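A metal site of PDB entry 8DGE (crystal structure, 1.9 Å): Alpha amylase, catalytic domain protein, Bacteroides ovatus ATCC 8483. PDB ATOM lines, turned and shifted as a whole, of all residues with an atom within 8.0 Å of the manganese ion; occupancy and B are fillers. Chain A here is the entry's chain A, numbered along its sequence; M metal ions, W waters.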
ATOM      1  N   TYR A 383      -3.255   4.913 -28.312  1.00  0.00           N
ATOM      2  CA  TYR A 383      -3.193   4.692 -26.842  1.00  0.00           C
ATOM      3  C   TYR A 383      -3.535   5.981 -26.080  1.00  0.00           C
ATOM      4  O   TYR A 383      -3.643   5.895 -24.871  1.00  0.00           O
ATOM      5  CB  TYR A 383      -1.848   4.120 -26.417  1.00  0.00           C
ATOM      6  CG  TYR A 383      -1.529   2.746 -26.961  1.00  0.00           C
ATOM      7  CD1 TYR A 383      -2.237   1.622 -26.562  1.00  0.00           C
ATOM      8  CD2 TYR A 383      -0.480   2.570 -27.857  1.00  0.00           C
ATOM      9  CE1 TYR A 383      -1.935   0.367 -27.058  1.00  0.00           C
ATOM     10  CE2 TYR A 383      -0.175   1.322 -28.364  1.00  0.00           C
ATOM     11  CZ  TYR A 383      -0.900   0.210 -27.970  1.00  0.00           C
ATOM     12  OH  TYR A 383      -0.561  -1.012 -28.477  1.00  0.00           O
ATOM     13  N   ASN A 384      -3.719   7.117 -26.746  1.00  0.00           N
ATOM     14  CA  ASN A 384      -4.208   8.336 -26.068  1.00  0.00           C
ATOM     15  C   ASN A 384      -5.551   8.045 -25.392  1.00  0.00           C
ATOM     16  O   ASN A 384      -5.706   8.374 -24.217  1.00  0.00           O
ATOM     17  CB  ASN A 384      -4.447   9.520 -26.999  1.00  0.00           C
ATOM     18  CG  ASN A 384      -5.141  10.645 -26.262  1.00  0.00           C
ATOM     19  OD1 ASN A 384      -4.561  11.211 -25.344  1.00  0.00           O
ATOM     20  ND2 ASN A 384      -6.376  10.929 -26.626  1.00  0.00           N
ATOM     21  N   HIS A 385      -6.493   7.454 -26.131  1.00  0.00           N
ATOM     22  CA  HIS A 385      -7.910   7.287 -25.720  1.00  0.00           C
ATOM     23  C   HIS A 385      -8.455   5.959 -26.234  1.00  0.00           C
ATOM     24  O   HIS A 385      -7.894   5.434 -27.205  1.00  0.00           O
ATOM     25  CB  HIS A 385      -8.754   8.459 -26.237  1.00  0.00           C
ATOM     26  CG  HIS A 385      -8.782   8.514 -27.721  1.00  0.00           C
ATOM     27  ND1 HIS A 385      -7.736   9.024 -28.455  1.00  0.00           N
ATOM     28  CD2 HIS A 385      -9.715   8.097 -28.612  1.00  0.00           C
ATOM     29  CE1 HIS A 385      -8.022   8.921 -29.737  1.00  0.00           C
ATOM     30  NE2 HIS A 385      -9.231   8.365 -29.866  1.00  0.00           N
ATOM     31  N   ASN A 412      -8.756   8.497 -16.939  1.00  0.00           N
ATOM     32  CA  ASN A 412      -9.171   9.759 -16.289  1.00  0.00           C
ATOM     33  C   ASN A 412     -10.692   9.888 -16.423  1.00  0.00           C
ATOM     34  O   ASN A 412     -11.229   9.436 -17.454  1.00  0.00           O
ATOM     35  CB  ASN A 412      -8.426  10.947 -16.906  1.00  0.00           C
ATOM     36  CG  ASN A 412      -6.915  10.846 -16.801  1.00  0.00           C
ATOM     37  OD1 ASN A 412      -6.372  10.757 -15.692  1.00  0.00           O
ATOM     38  ND2 ASN A 412      -6.215  10.871 -17.923  1.00  0.00           N
ATOM     39  N   THR A 415     -10.663  14.485 -19.286  1.00  0.00           N
ATOM     40  CA  THR A 415      -9.435  14.673 -20.092  1.00  0.00           C
ATOM     41  C   THR A 415      -8.645  15.841 -19.496  1.00  0.00           C
ATOM     42  O   THR A 415      -9.194  16.934 -19.353  1.00  0.00           O
ATOM     43  CB  THR A 415      -9.780  14.902 -21.566  1.00  0.00           C
ATOM     44  OG1 THR A 415     -10.619  13.819 -21.970  1.00  0.00           O
ATOM     45  CG2 THR A 415      -8.548  14.978 -22.454  1.00  0.00           C
ATOM     46  N   PRO A 416      -7.362  15.647 -19.101  1.00  0.00           N
ATOM     47  CA  PRO A 416      -6.526  16.743 -18.627  1.00  0.00           C
ATOM     48  C   PRO A 416      -6.184  17.769 -19.714  1.00  0.00           C
ATOM     49  O   PRO A 416      -6.092  18.933 -19.388  1.00  0.00           O
ATOM     50  CB  PRO A 416      -5.228  16.067 -18.130  1.00  0.00           C
ATOM     51  CG  PRO A 416      -5.553  14.581 -18.049  1.00  0.00           C
ATOM     52  CD  PRO A 416      -6.655  14.355 -19.067  1.00  0.00           C
ATOM     53  N   HIS A 417      -5.987  17.311 -20.972  1.00  0.00           N
ATOM     54  CA  HIS A 417      -5.688  18.170 -22.150  1.00  0.00           C
ATOM     55  C   HIS A 417      -7.006  18.556 -22.848  1.00  0.00           C
ATOM     56  O   HIS A 417      -7.397  17.876 -23.812  1.00  0.00           O
ATOM     57  CB  HIS A 417      -4.667  17.529 -23.111  1.00  0.00           C
ATOM     58  CG  HIS A 417      -4.874  16.076 -23.403  1.00  0.00           C
ATOM     59  ND1 HIS A 417      -5.891  15.628 -24.210  1.00  0.00           N
ATOM     60  CD2 HIS A 417      -4.208  14.972 -22.991  1.00  0.00           C
ATOM     61  CE1 HIS A 417      -5.853  14.310 -24.283  1.00  0.00           C
ATOM     62  NE2 HIS A 417      -4.831  13.886 -23.560  1.00  0.00           N
ATOM     63  N   TYR A 420      -7.948  18.751 -26.698  1.00  0.00           N
ATOM     64  CA  TYR A 420      -8.058  17.508 -27.523  1.00  0.00           C
ATOM     65  C   TYR A 420      -8.760  16.400 -26.725  1.00  0.00           C
ATOM     66  O   TYR A 420      -8.096  15.661 -25.989  1.00  0.00           O
ATOM     67  CB  TYR A 420      -6.675  17.111 -28.042  1.00  0.00           C
ATOM     68  CG  TYR A 420      -6.084  18.195 -28.917  1.00  0.00           C
ATOM     69  CD1 TYR A 420      -6.525  18.368 -30.219  1.00  0.00           C
ATOM     70  CD2 TYR A 420      -5.148  19.081 -28.422  1.00  0.00           C
ATOM     71  CE1 TYR A 420      -6.004  19.365 -31.016  1.00  0.00           C
ATOM     72  CE2 TYR A 420      -4.616  20.086 -29.218  1.00  0.00           C
ATOM     73  CZ  TYR A 420      -5.059  20.237 -30.509  1.00  0.00           C
ATOM     74  OH  TYR A 420      -4.563  21.232 -31.306  1.00  0.00           O
ATOM     75  N   PHE A 422     -10.955  13.367 -27.826  1.00  0.00           N
ATOM     76  CA  PHE A 422     -11.362  12.547 -28.994  1.00  0.00           C
ATOM     77  C   PHE A 422     -12.438  11.533 -28.564  1.00  0.00           C
ATOM     78  O   PHE A 422     -13.179  11.043 -29.436  1.00  0.00           O
ATOM     79  CB  PHE A 422     -10.143  11.886 -29.636  1.00  0.00           C
ATOM     80  CG  PHE A 422      -9.109  12.874 -30.114  1.00  0.00           C
ATOM     81  CD1 PHE A 422      -9.326  13.637 -31.242  1.00  0.00           C
ATOM     82  CD2 PHE A 422      -7.919  13.051 -29.419  1.00  0.00           C
ATOM     83  CE1 PHE A 422      -8.383  14.544 -31.687  1.00  0.00           C
ATOM     84  CE2 PHE A 422      -6.967  13.959 -29.870  1.00  0.00           C
ATOM     85  CZ  PHE A 422      -7.202  14.699 -31.011  1.00  0.00           C
ATOM     86  N   ASP A 425     -12.862   8.830 -22.879  1.00  0.00           N
ATOM     87  CA  ASP A 425     -12.053   7.738 -22.257  1.00  0.00           C
ATOM     88  C   ASP A 425     -10.558   7.975 -22.527  1.00  0.00           C
ATOM     89  O   ASP A 425      -9.960   7.173 -23.260  1.00  0.00           O
ATOM     90  CB  ASP A 425     -12.516   6.369 -22.748  1.00  0.00           C
ATOM     91  CG  ASP A 425     -14.017   6.218 -22.580  1.00  0.00           C
ATOM     92  OD1 ASP A 425     -14.446   6.107 -21.433  1.00  0.00           O
ATOM     93  OD2 ASP A 425     -14.733   6.302 -23.605  1.00  0.00           O
ATOM     94  N   ASP A 426      -9.996   8.997 -21.879  1.00  0.00           N
ATOM     95  CA  ASP A 426      -8.561   9.381 -21.946  1.00  0.00           C
ATOM     96  C   ASP A 426      -7.761   8.448 -21.027  1.00  0.00           C
ATOM     97  O   ASP A 426      -8.117   8.343 -19.844  1.00  0.00           O
ATOM     98  CB  ASP A 426      -8.385  10.836 -21.521  1.00  0.00           C
ATOM     99  CG  ASP A 426      -6.931  11.264 -21.552  1.00  0.00           C
ATOM    100  OD1 ASP A 426      -6.348  11.185 -22.649  1.00  0.00           O
ATOM    101  OD2 ASP A 426      -6.402  11.630 -20.494  1.00  0.00           O
ATOM    102  N   PHE A 427      -6.715   7.817 -21.560  1.00  0.00           N
ATOM    103  CA  PHE A 427      -5.785   6.928 -20.800  1.00  0.00           C
ATOM    104  C   PHE A 427      -4.898   7.781 -19.884  1.00  0.00           C
ATOM    105  O   PHE A 427      -4.313   8.786 -20.322  1.00  0.00           O
ATOM    106  CB  PHE A 427      -4.970   6.052 -21.744  1.00  0.00           C
ATOM    107  CG  PHE A 427      -5.578   4.707 -22.052  1.00  0.00           C
ATOM    108  CD1 PHE A 427      -5.730   3.759 -21.047  1.00  0.00           C
ATOM    109  CD2 PHE A 427      -5.997   4.378 -23.333  1.00  0.00           C
ATOM    110  CE1 PHE A 427      -6.291   2.518 -21.324  1.00  0.00           C
ATOM    111  CE2 PHE A 427      -6.563   3.143 -23.598  1.00  0.00           C
ATOM    112  CZ  PHE A 427      -6.695   2.204 -22.599  1.00  0.00           C
ATOM    113  N   ASN A 428      -4.806   7.380 -18.613  1.00  0.00           N
ATOM    114  CA  ASN A 428      -3.834   7.920 -17.627  1.00  0.00           C
ATOM    115  C   ASN A 428      -2.507   7.179 -17.806  1.00  0.00           C
ATOM    116  O   ASN A 428      -2.406   6.044 -17.298  1.00  0.00           O
ATOM    117  CB  ASN A 428      -4.387   7.813 -16.198  1.00  0.00           C
ATOM    118  CG  ASN A 428      -3.396   8.241 -15.133  1.00  0.00           C
ATOM    119  OD1 ASN A 428      -2.315   8.748 -15.427  1.00  0.00           O
ATOM    120  ND2 ASN A 428      -3.753   8.015 -13.882  1.00  0.00           N
ATOM    121  N   HIS A 429      -1.525   7.788 -18.476  1.00  0.00           N
ATOM    122  CA  HIS A 429      -0.223   7.145 -18.815  1.00  0.00           C
ATOM    123  C   HIS A 429       0.789   7.240 -17.668  1.00  0.00           C
ATOM    124  O   HIS A 429       1.933   6.799 -17.868  1.00  0.00           O
ATOM    125  CB  HIS A 429       0.324   7.727 -20.138  1.00  0.00           C
ATOM    126  CG  HIS A 429      -0.411   7.192 -21.329  1.00  0.00           C
ATOM    127  ND1 HIS A 429      -0.092   5.975 -21.899  1.00  0.00           N
ATOM    128  CD2 HIS A 429      -1.468   7.676 -22.005  1.00  0.00           C
ATOM    129  CE1 HIS A 429      -0.916   5.749 -22.902  1.00  0.00           C
ATOM    130  NE2 HIS A 429      -1.780   6.777 -22.977  1.00  0.00           N
ATOM    131  N   PHE A 458      -1.047  10.526 -31.776  1.00  0.00           N
ATOM    132  CA  PHE A 458      -1.241  11.628 -30.796  1.00  0.00           C
ATOM    133  C   PHE A 458      -0.496  11.373 -29.473  1.00  0.00           C
ATOM    134  O   PHE A 458      -1.163  11.317 -28.432  1.00  0.00           O
ATOM    135  CB  PHE A 458      -2.736  11.825 -30.489  1.00  0.00           C
ATOM    136  CG  PHE A 458      -3.074  13.087 -29.728  1.00  0.00           C
ATOM    137  CD1 PHE A 458      -2.686  14.328 -30.199  1.00  0.00           C
ATOM    138  CD2 PHE A 458      -3.842  13.033 -28.567  1.00  0.00           C
ATOM    139  CE1 PHE A 458      -3.001  15.487 -29.491  1.00  0.00           C
ATOM    140  CE2 PHE A 458      -4.164  14.190 -27.871  1.00  0.00           C
ATOM    141  CZ  PHE A 458      -3.750  15.420 -28.342  1.00  0.00           C
ATOM    142  N   THR A 459       0.830  11.254 -29.515  1.00  0.00           N
ATOM    143  CA  THR A 459       1.659  10.995 -28.301  1.00  0.00           C
ATOM    144  C   THR A 459       1.729  12.269 -27.459  1.00  0.00           C
ATOM    145  O   THR A 459       2.036  12.176 -26.267  1.00  0.00           O
ATOM    146  CB  THR A 459       3.046  10.454 -28.661  1.00  0.00           C
ATOM    147  OG1 THR A 459       3.642  11.375 -29.573  1.00  0.00           O
ATOM    148  CG2 THR A 459       2.993   9.064 -29.250  1.00  0.00           C
ATOM    149  N   LYS A 460       1.413  13.425 -28.045  1.00  0.00           N
ATOM    150  CA  LYS A 460       1.198  14.686 -27.300  1.00  0.00           C
ATOM    151  C   LYS A 460       0.126  14.452 -26.221  1.00  0.00           C
ATOM    152  O   LYS A 460       0.174  15.145 -25.169  1.00  0.00           O
ATOM    153  CB  LYS A 460       0.780  15.781 -28.292  1.00  0.00           C
ATOM    154  CG  LYS A 460       0.415  17.120 -27.680  1.00  0.00           C
ATOM    155  CD  LYS A 460       0.021  18.147 -28.720  1.00  0.00           C
ATOM    156  CE  LYS A 460       1.209  18.644 -29.498  1.00  0.00           C
ATOM    157  NZ  LYS A 460       0.804  19.663 -30.503  1.00  0.00           N
ATOM    158  N   GLY A 461      -0.809  13.520 -26.439  1.00  0.00           N
ATOM    159  CA  GLY A 461      -1.911  13.200 -25.507  1.00  0.00           C
ATOM    160  C   GLY A 461      -1.468  12.424 -24.283  1.00  0.00           C
ATOM    161  O   GLY A 461      -2.269  12.292 -23.343  1.00  0.00           O
ATOM    162  N   PHE A 462      -0.236  11.904 -24.246  1.00  0.00           N
ATOM    163  CA  PHE A 462       0.220  11.017 -23.146  1.00  0.00           C
ATOM    164  C   PHE A 462       0.671  11.885 -21.959  1.00  0.00           C
ATOM    165  O   PHE A 462       1.862  11.818 -21.603  1.00  0.00           O
ATOM    166  CB  PHE A 462       1.346  10.081 -23.614  1.00  0.00           C
ATOM    167  CG  PHE A 462       0.932   9.023 -24.619  1.00  0.00           C
ATOM    168  CD1 PHE A 462       1.596   7.805 -24.653  1.00  0.00           C
ATOM    169  CD2 PHE A 462      -0.091   9.251 -25.535  1.00  0.00           C
ATOM    170  CE1 PHE A 462       1.241   6.844 -25.592  1.00  0.00           C
ATOM    171  CE2 PHE A 462      -0.421   8.292 -26.474  1.00  0.00           C
ATOM    172  CZ  PHE A 462       0.241   7.088 -26.490  1.00  0.00           C
ATOM    173  N   THR A 463      -0.258  12.640 -21.359  1.00  0.00           N
ATOM    174  CA  THR A 463       0.038  13.679 -20.350  1.00  0.00           C
ATOM    175  C   THR A 463      -1.111  13.808 -19.341  1.00  0.00           C
ATOM    176  O   THR A 463      -2.287  13.736 -19.751  1.00  0.00           O
ATOM    177  CB  THR A 463       0.371  15.018 -21.028  1.00  0.00           C
ATOM    178  OG1 THR A 463       0.678  15.994 -20.032  1.00  0.00           O
ATOM    179  CG2 THR A 463      -0.729  15.508 -21.942  1.00  0.00           C
ATOM    180  N   GLN A 464      -0.764  13.996 -18.063  1.00  0.00           N
ATOM    181  CA  GLN A 464      -1.728  14.192 -16.953  1.00  0.00           C
ATOM    182  C   GLN A 464      -1.850  15.689 -16.652  1.00  0.00           C
ATOM    183  O   GLN A 464      -2.761  16.053 -15.896  1.00  0.00           O
ATOM    184  CB  GLN A 464      -1.294  13.380 -15.730  1.00  0.00           C
ATOM    185  CG  GLN A 464      -1.514  11.881 -15.925  1.00  0.00           C
ATOM    186  CD  GLN A 464      -2.958  11.559 -16.216  1.00  0.00           C
ATOM    187  OE1 GLN A 464      -3.328  11.289 -17.363  1.00  0.00           O
ATOM    188  NE2 GLN A 464      -3.789  11.585 -15.187  1.00  0.00           N
ATOM    189  N   LEU A 473      -0.135  22.611 -23.590  1.00  0.00           N
ATOM    190  CA  LEU A 473      -0.014  21.179 -23.987  1.00  0.00           C
ATOM    191  C   LEU A 473       1.375  20.934 -24.613  1.00  0.00           C
ATOM    192  O   LEU A 473       2.039  19.966 -24.216  1.00  0.00           O
ATOM    193  CB  LEU A 473      -1.143  20.843 -24.955  1.00  0.00           C
ATOM    194  CG  LEU A 473      -1.191  19.395 -25.458  1.00  0.00           C
ATOM    195  CD1 LEU A 473      -1.077  18.401 -24.324  1.00  0.00           C
ATOM    196  CD2 LEU A 473      -2.467  19.147 -26.254  1.00  0.00           C
HETATM  197 MN    MN M   1      -4.360  11.709 -23.058  1.00  0.00          MN
HETATM  198  O   HOH W   1      -3.963   9.656 -22.803  1.00  0.00           O
HETATM  199  O   HOH W   2      -3.979  12.036 -20.893  1.00  0.00           O
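Water W1 lies within hydrogen-bond range of O of Asn 384 (2.6 Å) and O of Phe 427 (2.7 Å).
OD1 of Asp 426 binds the manganese ion (2.1 Å).
Water W1 binds the manganese ion, 2.1 Å away.
O of Gly 461 binds the manganese ion, 2.2 Å away.
Water W2 binds the manganese ion (2.2 Å).
NE2 of His 417 is bound to the manganese ion.
The side-chain amide oxygen (OD1) of Asn 384 binds the manganese ion, 2.3 Å away.
The manganese ion has six donor atoms within binding distance.
The backbone carbonyl oxygen (O) of Asn 384 lies within hydrogen-bond range of the backbone NH (N) of Phe 427 (2.9 Å).
ND2 of Asn 412 sits at hydrogen-bond distance from OD2 of Asp 426.
O of Tyr 420 lies within hydrogen-bond range of ND1 of His 417.
The side-chain amide nitrogen (ND2) of Asn 384 is in hydrogen-bond range of a ring nitrogen (ND1) of His 385 (3.0 Å).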
